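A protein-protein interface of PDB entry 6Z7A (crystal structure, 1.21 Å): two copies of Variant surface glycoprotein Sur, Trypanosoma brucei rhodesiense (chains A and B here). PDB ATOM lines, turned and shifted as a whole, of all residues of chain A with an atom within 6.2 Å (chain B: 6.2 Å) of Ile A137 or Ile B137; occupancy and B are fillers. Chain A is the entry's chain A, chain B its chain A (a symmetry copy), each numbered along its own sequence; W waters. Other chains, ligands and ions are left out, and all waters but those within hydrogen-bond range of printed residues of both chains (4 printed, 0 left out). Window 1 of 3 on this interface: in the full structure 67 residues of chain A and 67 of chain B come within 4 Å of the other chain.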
ATOM      1  N   SER A 132      17.755  28.886  -4.413  1.00  0.00           N
ATOM      2  CA  SER A 132      18.922  28.012  -4.430  1.00  0.00           C
ATOM      3  C   SER A 132      19.485  27.815  -3.036  1.00  0.00           C
ATOM      4  O   SER A 132      19.935  26.732  -2.668  1.00  0.00           O
ATOM      5  CB  SER A 132      19.949  28.570  -5.404  1.00  0.00           C
ATOM      6  OG  SER A 132      20.729  29.563  -4.804  1.00  0.00           O
ATOM      7  N   ALA A 133      19.511  28.884  -2.221  1.00  0.00           N
ATOM      8  CA  ALA A 133      19.977  28.803  -0.865  1.00  0.00           C
ATOM      9  C   ALA A 133      19.063  27.958  -0.023  1.00  0.00           C
ATOM     10  O   ALA A 133      19.497  27.142   0.809  1.00  0.00           O
ATOM     11  CB  ALA A 133      20.172  30.231  -0.303  1.00  0.00           C
ATOM     12  N   ALA A 134      17.769  28.140  -0.192  1.00  0.00           N
ATOM     13  CA  ALA A 134      16.816  27.300   0.497  1.00  0.00           C
ATOM     14  C   ALA A 134      16.952  25.849   0.124  1.00  0.00           C
ATOM     15  O   ALA A 134      16.815  24.983   0.977  1.00  0.00           O
ATOM     16  CB  ALA A 134      15.401  27.844   0.258  1.00  0.00           C
ATOM     17  N   LEU A 135      17.117  25.570  -1.166  1.00  0.00           N
ATOM     18  CA  LEU A 135      17.307  24.197  -1.653  1.00  0.00           C
ATOM     19  C   LEU A 135      18.456  23.544  -0.922  1.00  0.00           C
ATOM     20  O   LEU A 135      18.343  22.371  -0.495  1.00  0.00           O
ATOM     21  CB  LEU A 135      17.482  24.222  -3.141  1.00  0.00           C
ATOM     22  CG  LEU A 135      17.627  22.909  -3.852  1.00  0.00           C
ATOM     23  CD1 LEU A 135      17.405  23.163  -5.312  1.00  0.00           C
ATOM     24  CD2 LEU A 135      19.036  22.440  -3.726  1.00  0.00           C
ATOM     25  N   GLN A 136      19.564  24.248  -0.737  1.00  0.00           N
ATOM     26  CA  GLN A 136      20.685  23.629  -0.051  1.00  0.00           C
ATOM     27  C   GLN A 136      20.330  23.227   1.354  1.00  0.00           C
ATOM     28  O   GLN A 136      20.696  22.144   1.839  1.00  0.00           O
ATOM     29  CB  GLN A 136      21.882  24.571  -0.100  1.00  0.00           C
ATOM     30  CG  GLN A 136      23.133  24.081   0.620  1.00  0.00           C
ATOM     31  CD  GLN A 136      23.753  22.847  -0.052  1.00  0.00           C
ATOM     32  OE1 GLN A 136      23.892  22.820  -1.274  1.00  0.00           O
ATOM     33  NE2 GLN A 136      24.088  21.852   0.732  1.00  0.00           N
ATOM     34  N   ILE A 137      19.606  24.117   2.092  1.00  0.00           N
ATOM     35  CA  ILE A 137      19.212  23.788   3.459  1.00  0.00           C
ATOM     36  C   ILE A 137      18.143  22.684   3.513  1.00  0.00           C
ATOM     37  O   ILE A 137      18.212  21.817   4.382  1.00  0.00           O
ATOM     38  CB  ILE A 137      18.775  25.078   4.183  1.00  0.00           C
ATOM     39  CG1 ILE A 137      19.987  26.004   4.393  1.00  0.00           C
ATOM     40  CG2 ILE A 137      18.109  24.705   5.541  1.00  0.00           C
ATOM     41  CD1 ILE A 137      19.665  27.446   4.779  1.00  0.00           C
ATOM     42  N   GLN A 138      17.180  22.699   2.606  1.00  0.00           N
ATOM     43  CA  GLN A 138      16.124  21.711   2.634  1.00  0.00           C
ATOM     44  C   GLN A 138      16.619  20.349   2.196  1.00  0.00           C
ATOM     45  O   GLN A 138      15.960  19.372   2.465  1.00  0.00           O
ATOM     46  CB  GLN A 138      14.940  22.143   1.765  1.00  0.00           C
ATOM     47  CG  GLN A 138      14.235  23.438   2.230  1.00  0.00           C
ATOM     48  CD  GLN A 138      13.594  23.315   3.588  1.00  0.00           C
ATOM     49  OE1 GLN A 138      13.553  22.262   4.198  1.00  0.00           O
ATOM     50  NE2 GLN A 138      13.051  24.441   4.060  1.00  0.00           N
ATOM     51  N   ALA A 139      17.838  20.269   1.648  1.00  0.00           N
ATOM     52  CA  ALA A 139      18.458  18.993   1.350  1.00  0.00           C
ATOM     53  C   ALA A 139      19.126  18.354   2.573  1.00  0.00           C
ATOM     54  O   ALA A 139      19.573  17.184   2.473  1.00  0.00           O
ATOM     55  CB  ALA A 139      19.534  19.177   0.272  1.00  0.00           C
ATOM     56  N   ALA A 140      19.227  19.088   3.660  1.00  0.00           N
ATOM     57  CA  ALA A 140      19.851  18.573   4.867  1.00  0.00           C
ATOM     58  C   ALA A 140      18.867  17.701   5.644  1.00  0.00           C
ATOM     59  O   ALA A 140      18.109  18.195   6.513  1.00  0.00           O
ATOM     60  CB  ALA A 140      20.396  19.716   5.697  1.00  0.00           C
ATOM     61  N   GLN A 141      18.756  16.441   5.228  1.00  0.00           N
ATOM     62  CA  GLN A 141      17.683  15.572   5.604  1.00  0.00           C
ATOM     63  C   GLN A 141      18.023  14.451   6.533  1.00  0.00           C
ATOM     64  O   GLN A 141      17.099  13.704   6.981  1.00  0.00           O
ATOM     65  CB  GLN A 141      17.031  15.055   4.332  1.00  0.00           C
ATOM     66  CG  GLN A 141      16.429  16.194   3.531  1.00  0.00           C
ATOM     67  CD  GLN A 141      15.541  15.738   2.412  1.00  0.00           C
ATOM     68  OE1 GLN A 141      15.238  14.539   2.291  1.00  0.00           O
ATOM     69  NE2 GLN A 141      15.025  16.690   1.689  1.00  0.00           N
ATOM     70  N   ALA A 171      22.219  18.771  10.942  1.00  0.00           N
ATOM     71  CA  ALA A 171      21.929  18.197   9.632  1.00  0.00           C
ATOM     72  C   ALA A 171      22.556  19.082   8.604  1.00  0.00           C
ATOM     73  O   ALA A 171      22.346  20.294   8.596  1.00  0.00           O
ATOM     74  CB  ALA A 171      20.444  17.988   9.370  1.00  0.00           C
ATOM     75  N   ALA A 173      23.812  18.837   4.198  1.00  0.00           N
ATOM     76  CA  ALA A 173      23.895  18.107   2.938  1.00  0.00           C
ATOM     77  C   ALA A 173      25.210  18.437   2.265  1.00  0.00           C
ATOM     78  O   ALA A 173      25.750  19.526   2.440  1.00  0.00           O
ATOM     79  CB  ALA A 173      22.722  18.435   2.027  1.00  0.00           C
ATOM     80  N   TYR A 208       8.848  26.585   1.886  1.00  0.00           N
ATOM     81  CA  TYR A 208      10.176  26.032   1.549  1.00  0.00           C
ATOM     82  C   TYR A 208      11.309  26.976   1.929  1.00  0.00           C
ATOM     83  O   TYR A 208      12.441  26.548   2.159  1.00  0.00           O
ATOM     84  CB  TYR A 208      10.157  25.746   0.069  1.00  0.00           C
ATOM     85  CG  TYR A 208      11.293  24.869  -0.441  1.00  0.00           C
ATOM     86  CD1 TYR A 208      11.267  23.511  -0.253  1.00  0.00           C
ATOM     87  CD2 TYR A 208      12.329  25.419  -1.128  1.00  0.00           C
ATOM     88  CE1 TYR A 208      12.220  22.696  -0.762  1.00  0.00           C
ATOM     89  CE2 TYR A 208      13.388  24.633  -1.648  1.00  0.00           C
ATOM     90  CZ  TYR A 208      13.252  23.271  -1.441  1.00  0.00           C
ATOM     91  OH  TYR A 208      14.272  22.482  -2.001  1.00  0.00           O
ATOM     92  N   LEU A 209      11.015  28.262   1.903  1.00  0.00           N
ATOM     93  CA  LEU A 209      11.958  29.311   2.217  1.00  0.00           C
ATOM     94  C   LEU A 209      12.077  29.578   3.732  1.00  0.00           C
ATOM     95  O   LEU A 209      13.112  30.067   4.189  1.00  0.00           O
ATOM     96  CB  LEU A 209      11.579  30.646   1.492  1.00  0.00           C
ATOM     97  CG  LEU A 209      11.827  30.851  -0.013  1.00  0.00           C
ATOM     98  CD1 LEU A 209      13.249  31.166  -0.278  1.00  0.00           C
ATOM     99  CD2 LEU A 209      11.359  29.757  -0.866  1.00  0.00           C
ATOM    100  N   THR A 210      11.024  29.263   4.496  1.00  0.00           N
ATOM    101  CA  THR A 210      10.882  29.715   5.874  1.00  0.00           C
ATOM    102  C   THR A 210      10.935  28.642   6.947  1.00  0.00           C
ATOM    103  O   THR A 210      11.133  28.973   8.122  1.00  0.00           O
ATOM    104  CB  THR A 210       9.580  30.488   6.049  1.00  0.00           C
ATOM    105  OG1 THR A 210       8.511  29.568   5.923  1.00  0.00           O
ATOM    106  CG2 THR A 210       9.471  31.648   5.025  1.00  0.00           C
ATOM    107  N   THR A 211      10.640  27.382   6.602  1.00  0.00           N
ATOM    108  CA  THR A 211      10.240  26.424   7.584  1.00  0.00           C
ATOM    109  C   THR A 211      11.178  25.229   7.580  1.00  0.00           C
ATOM    110  O   THR A 211      11.438  24.651   6.504  1.00  0.00           O
ATOM    111  CB  THR A 211       8.788  25.977   7.316  1.00  0.00           C
ATOM    112  OG1 THR A 211       7.948  27.131   7.450  1.00  0.00           O
ATOM    113  CG2 THR A 211       8.308  24.922   8.280  1.00  0.00           C
ATOM    114  N   ILE A 212      11.616  24.830   8.751  1.00  0.00           N
ATOM    115  CA  ILE A 212      12.321  23.569   9.008  1.00  0.00           C
ATOM    116  C   ILE A 212      11.275  22.549   9.431  1.00  0.00           C
ATOM    117  O   ILE A 212      10.415  22.840  10.269  1.00  0.00           O
ATOM    118  CB  ILE A 212      13.375  23.758  10.115  1.00  0.00           C
ATOM    119  CG1 ILE A 212      14.431  24.760   9.718  1.00  0.00           C
ATOM    120  CG2 ILE A 212      13.981  22.420  10.528  1.00  0.00           C
ATOM    121  CD1 ILE A 212      15.273  25.289  10.819  1.00  0.00           C
ATOM    122  N   GLY A 260      13.409  18.060   6.409  1.00  0.00           N
ATOM    123  CA  GLY A 260      13.212  18.605   5.087  1.00  0.00           C
ATOM    124  C   GLY A 260      11.750  18.991   4.881  1.00  0.00           C
ATOM    125  O   GLY A 260      10.836  18.220   5.219  1.00  0.00           O
ATOM    126  N   SER B 132      20.736  36.478   3.259  1.00  0.00           N
ATOM    127  CA  SER B 132      19.438  36.921   3.753  1.00  0.00           C
ATOM    128  C   SER B 132      18.463  35.765   3.859  1.00  0.00           C
ATOM    129  O   SER B 132      17.658  35.681   4.783  1.00  0.00           O
ATOM    130  CB  SER B 132      18.922  38.044   2.866  1.00  0.00           C
ATOM    131  OG  SER B 132      18.291  37.538   1.726  1.00  0.00           O
ATOM    132  N   ALA B 133      18.482  34.845   2.878  1.00  0.00           N
ATOM    133  CA  ALA B 133      17.639  33.683   2.898  1.00  0.00           C
ATOM    134  C   ALA B 133      18.013  32.756   4.020  1.00  0.00           C
ATOM    135  O   ALA B 133      17.158  32.188   4.722  1.00  0.00           O
ATOM    136  CB  ALA B 133      17.671  33.001   1.510  1.00  0.00           C
ATOM    137  N   ALA B 134      19.300  32.553   4.212  1.00  0.00           N
ATOM    138  CA  ALA B 134      19.757  31.761   5.332  1.00  0.00           C
ATOM    139  C   ALA B 134      19.359  32.353   6.656  1.00  0.00           C
ATOM    140  O   ALA B 134      19.010  31.622   7.572  1.00  0.00           O
ATOM    141  CB  ALA B 134      21.270  31.543   5.210  1.00  0.00           C
ATOM    142  N   LEU B 135      19.509  33.667   6.800  1.00  0.00           N
ATOM    143  CA  LEU B 135      19.116  34.371   8.027  1.00  0.00           C
ATOM    144  C   LEU B 135      17.675  34.064   8.360  1.00  0.00           C
ATOM    145  O   LEU B 135      17.347  33.789   9.537  1.00  0.00           O
ATOM    146  CB  LEU B 135      19.394  35.834   7.867  1.00  0.00           C
ATOM    147  CG  LEU B 135      19.122  36.732   9.038  1.00  0.00           C
ATOM    148  CD1 LEU B 135      19.818  38.034   8.774  1.00  0.00           C
ATOM    149  CD2 LEU B 135      17.666  37.046   9.083  1.00  0.00           C
ATOM    150  N   GLN B 136      16.786  34.081   7.376  1.00  0.00           N
ATOM    151  CA  GLN B 136      15.393  33.806   7.681  1.00  0.00           C
ATOM    152  C   GLN B 136      15.206  32.426   8.250  1.00  0.00           C
ATOM    153  O   GLN B 136      14.443  32.208   9.206  1.00  0.00           O
ATOM    154  CB  GLN B 136      14.553  34.037   6.431  1.00  0.00           C
ATOM    155  CG  GLN B 136      13.064  33.744   6.577  1.00  0.00           C
ATOM    156  CD  GLN B 136      12.365  34.720   7.536  1.00  0.00           C
ATOM    157  OE1 GLN B 136      12.585  35.927   7.451  1.00  0.00           O
ATOM    158  NE2 GLN B 136      11.567  34.195   8.435  1.00  0.00           N
ATOM    159  N   ILE B 137      15.890  31.409   7.653  1.00  0.00           N
ATOM    160  CA  ILE B 137      15.769  30.045   8.161  1.00  0.00           C
ATOM    161  C   ILE B 137      16.447  29.865   9.529  1.00  0.00           C
ATOM    162  O   ILE B 137      15.904  29.172  10.388  1.00  0.00           O
ATOM    163  CB  ILE B 137      16.300  29.061   7.098  1.00  0.00           C
ATOM    164  CG1 ILE B 137      15.366  29.050   5.874  1.00  0.00           C
ATOM    165  CG2 ILE B 137      16.420  27.640   7.727  1.00  0.00           C
ATOM    166  CD1 ILE B 137      15.929  28.399   4.612  1.00  0.00           C
ATOM    167  N   GLN B 138      17.601  30.477   9.743  1.00  0.00           N
ATOM    168  CA  GLN B 138      18.305  30.308  10.994  1.00  0.00           C
ATOM    169  C   GLN B 138      17.620  31.044  12.126  1.00  0.00           C
ATOM    170  O   GLN B 138      17.892  30.749  13.267  1.00  0.00           O
ATOM    171  CB  GLN B 138      19.761  30.768  10.876  1.00  0.00           C
ATOM    172  CG  GLN B 138      20.614  29.960   9.871  1.00  0.00           C
ATOM    173  CD  GLN B 138      20.777  28.513  10.253  1.00  0.00           C
ATOM    174  OE1 GLN B 138      20.361  28.065  11.306  1.00  0.00           O
ATOM    175  NE2 GLN B 138      21.435  27.764   9.363  1.00  0.00           N
ATOM    176  N   ALA B 139      16.636  31.899  11.816  1.00  0.00           N
ATOM    177  CA  ALA B 139      15.818  32.522  12.837  1.00  0.00           C
ATOM    178  C   ALA B 139      14.680  31.617  13.324  1.00  0.00           C
ATOM    179  O   ALA B 139      13.991  31.992  14.306  1.00  0.00           O
ATOM    180  CB  ALA B 139      15.190  33.809  12.286  1.00  0.00           C
ATOM    181  N   ALA B 140      14.464  30.505  12.657  1.00  0.00           N
ATOM    182  CA  ALA B 140      13.404  29.586  13.038  1.00  0.00           C
ATOM    183  C   ALA B 140      13.855  28.706  14.201  1.00  0.00           C
ATOM    184  O   ALA B 140      14.429  27.610  14.000  1.00  0.00           O
ATOM    185  CB  ALA B 140      12.961  28.780  11.836  1.00  0.00           C
ATOM    186  N   GLN B 141      13.747  29.249  15.414  1.00  0.00           N
ATOM    187  CA  GLN B 141      14.397  28.728  16.577  1.00  0.00           C
ATOM    188  C   GLN B 141      13.520  28.084  17.602  1.00  0.00           C
ATOM    189  O   GLN B 141      14.044  27.517  18.611  1.00  0.00           O
ATOM    190  CB  GLN B 141      15.231  29.843  17.187  1.00  0.00           C
ATOM    191  CG  GLN B 141      16.316  30.292  16.227  1.00  0.00           C
ATOM    192  CD  GLN B 141      17.339  31.191  16.856  1.00  0.00           C
ATOM    193  OE1 GLN B 141      17.338  31.392  18.082  1.00  0.00           O
ATOM    194  NE2 GLN B 141      18.274  31.615  16.055  1.00  0.00           N
ATOM    195  N   ALA B 171       9.511  24.379  12.513  1.00  0.00           N
ATOM    196  CA  ALA B 171      10.008  25.633  13.070  1.00  0.00           C
ATOM    197  C   ALA B 171       9.962  26.657  11.982  1.00  0.00           C
ATOM    198  O   ALA B 171      10.476  26.443  10.885  1.00  0.00           O
ATOM    199  CB  ALA B 171      11.396  25.522  13.685  1.00  0.00           C
ATOM    200  N   ALA B 173      10.023  31.229  11.595  1.00  0.00           N
ATOM    201  CA  ALA B 173      10.121  32.554  12.196  1.00  0.00           C
ATOM    202  C   ALA B 173       9.193  33.497  11.459  1.00  0.00           C
ATOM    203  O   ALA B 173       8.931  33.321  10.272  1.00  0.00           O
ATOM    204  CB  ALA B 173      11.552  33.071  12.170  1.00  0.00           C
ATOM    205  N   TYR B 208      26.497  28.442   8.412  1.00  0.00           N
ATOM    206  CA  TYR B 208      25.228  29.188   8.534  1.00  0.00           C
ATOM    207  C   TYR B 208      24.322  28.993   7.325  1.00  0.00           C
ATOM    208  O   TYR B 208      23.102  29.129   7.418  1.00  0.00           O
ATOM    209  CB  TYR B 208      25.601  30.636   8.727  1.00  0.00           C
ATOM    210  CG  TYR B 208      24.474  31.543   9.204  1.00  0.00           C
ATOM    211  CD1 TYR B 208      24.086  31.543  10.519  1.00  0.00           C
ATOM    212  CD2 TYR B 208      23.864  32.394   8.338  1.00  0.00           C
ATOM    213  CE1 TYR B 208      23.144  32.392  10.991  1.00  0.00           C
ATOM    214  CE2 TYR B 208      22.835  33.277   8.751  1.00  0.00           C
ATOM    215  CZ  TYR B 208      22.542  33.232  10.103  1.00  0.00           C
ATOM    216  OH  TYR B 208      21.560  34.143  10.528  1.00  0.00           O
ATOM    217  N   LEU B 209      24.938  28.763   6.180  1.00  0.00           N
ATOM    218  CA  LEU B 209      24.254  28.566   4.922  1.00  0.00           C
ATOM    219  C   LEU B 209      23.775  27.113   4.721  1.00  0.00           C
ATOM    220  O   LEU B 209      22.817  26.881   3.980  1.00  0.00           O
ATOM    221  CB  LEU B 209      25.164  28.975   3.716  1.00  0.00           C
ATOM    222  CG  LEU B 209      25.427  30.449   3.361  1.00  0.00           C
ATOM    223  CD1 LEU B 209      24.278  31.032   2.631  1.00  0.00           C
ATOM    224  CD2 LEU B 209      25.819  31.292   4.493  1.00  0.00           C
ATOM    225  N   THR B 210      24.439  26.151   5.372  1.00  0.00           N
ATOM    226  CA  THR B 210      24.287  24.735   5.062  1.00  0.00           C
ATOM    227  C   THR B 210      23.645  23.873   6.133  1.00  0.00           C
ATOM    228  O   THR B 210      23.208  22.757   5.828  1.00  0.00           O
ATOM    229  CB  THR B 210      25.637  24.120   4.712  1.00  0.00           C
ATOM    230  OG1 THR B 210      26.416  24.087   5.894  1.00  0.00           O
ATOM    231  CG2 THR B 210      26.340  24.910   3.577  1.00  0.00           C
ATOM    232  N   THR B 211      23.686  24.298   7.403  1.00  0.00           N
ATOM    233  CA  THR B 211      23.517  23.387   8.491  1.00  0.00           C
ATOM    234  C   THR B 211      22.342  23.802   9.359  1.00  0.00           C
ATOM    235  O   THR B 211      22.264  24.978   9.774  1.00  0.00           O
ATOM    236  CB  THR B 211      24.814  23.324   9.324  1.00  0.00           C
ATOM    237  OG1 THR B 211      25.851  22.816   8.474  1.00  0.00           O
ATOM    238  CG2 THR B 211      24.699  22.423  10.527  1.00  0.00           C
ATOM    239  N   ILE B 212      21.494  22.854   9.681  1.00  0.00           N
ATOM    240  CA  ILE B 212      20.440  22.967  10.695  1.00  0.00           C
ATOM    241  C   ILE B 212      21.011  22.430  11.998  1.00  0.00           C
ATOM    242  O   ILE B 212      21.635  21.363  12.019  1.00  0.00           O
ATOM    243  CB  ILE B 212      19.197  22.161  10.272  1.00  0.00           C
ATOM    244  CG1 ILE B 212      18.604  22.679   8.986  1.00  0.00           C
ATOM    245  CG2 ILE B 212      18.169  22.110  11.398  1.00  0.00           C
ATOM    246  CD1 ILE B 212      17.648  21.775   8.300  1.00  0.00           C
ATOM    247  N   GLY B 260      18.748  26.495  15.489  1.00  0.00           N
ATOM    248  CA  GLY B 260      19.457  27.631  14.950  1.00  0.00           C
ATOM    249  C   GLY B 260      20.963  27.390  14.994  1.00  0.00           C
ATOM    250  O   GLY B 260      21.504  26.934  16.016  1.00  0.00           O
HETATM  251  O   HOH W   1      14.803  31.884   3.122  1.00  0.00           O
HETATM  252  O   HOH W   2      22.891  21.598   3.445  1.00  0.00           O
HETATM  253  O   HOH W   3      11.814  31.325   9.182  1.00  0.00           O
HETATM  254  O   HOH W   4      22.049  28.093   1.691  1.00  0.00           O
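N of Ala A171 lies within hydrogen-bond range of O of Ile B212.
The backbone carbonyl oxygen (O) of Ile A212 is in hydrogen-bond range of the backbone NH (N) of Ala B171, at 2.9 Å.
Of the 18 printed residues of chain A, 6 touch a printed residue of chain B.
Hydrophobic or aromatic side chains of chain B within 4 Å of the printed part of chain A: Ile B137 and Ile B212.
Among the printed residues, no Asp or Glu carboxylate lies within 4 Å of a Lys or Arg side-chain nitrogen of the other chain.
The backbone carbonyl oxygen (O) of Thr A211 is in hydrogen-bond range of the side-chain amide nitrogen (NE2) of Gln A138 (2.9 Å).
The side-chain hydroxyl (OG1) of Thr A210 lies within hydrogen-bond range of the side-chain hydroxyl (OG1) of Thr A211.
NE2 of Gln B138 sits at hydrogen-bond distance from O of Thr B211, 2.9 Å away.
The side-chain hydroxyl (OG1) of Thr B210 lies within hydrogen-bond range of the side-chain hydroxyl (OG1) of Thr B211 (2.9 Å).
Printed residues of chain B within 4 Å of Ile A137: Ile B137 (3.9 Å), Leu B209 (3.0 Å) and Ile B212 (3.96 Å).
Printed residues of chain A within 4 Å of Ile B137: Ile A137, Leu A209 and Ile A212.
Of the printed residues of chain A, Ile B212 touches Ile A137 (3.96 Å) and Ala A171 (2.9 Å).
Printed residues of chain A within 4 Å of Thr B211: Ala A171 (3.3 Å).
Of the printed residues of chain B, Thr A210 touches Ala B171.
Of the printed residues of chain B, Ala A171 touches Thr B210 (3.8 Å), Thr B211 (3.3 Å) and Ile B212 (2.9 Å).
Ile A137 touches its own counterpart, Ile B137.
Ile A137 touches Leu B209, and with the chains exchanged Leu A209 touches Ile B137.
Ala A171 touches Thr B210, and with the chains exchanged Thr A210 touches Ala B171.
Ala A171 touches Ile B212, and with the chains exchanged Ile A212 touches Ala B171.
Ile A137 touches Ile B137.
Leu B209 touches Ile A137.
Ile A137 touches Ile B212.
Ala A171 touches Thr B210.
O of Ala A171 touches CA of Thr B211 (3.3 Å).
Leu A209 touches Ile B137 (O to CG1, 3.0 Å).
Ala B171 touches Thr A210 (O to O, 3.8 Å).
O of Ala B171 touches CA of Thr A211 (3.3 Å).
O of Ile B137 touches CD1 of Ile A212, at 3.96 Å.
Water W3 lies within hydrogen-bond range of O of Thr A210, O of Gln B136 and N of Ala B173.
Water W2 lies within hydrogen-bond range of O of Thr B210 (2.7 Å), O of Gln A136 (2.8 Å) and N of Ala A173 (3.0 Å).
Water W1 bridges the backbone carbonyl oxygen of Leu A209 (2.7 Å) and the backbone carbonyl oxygen of Ala B133 (2.9 Å).
Water W4 lies within hydrogen-bond range of O of Leu B209 (2.7 Å) and O of Ala A133 (2.9 Å).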
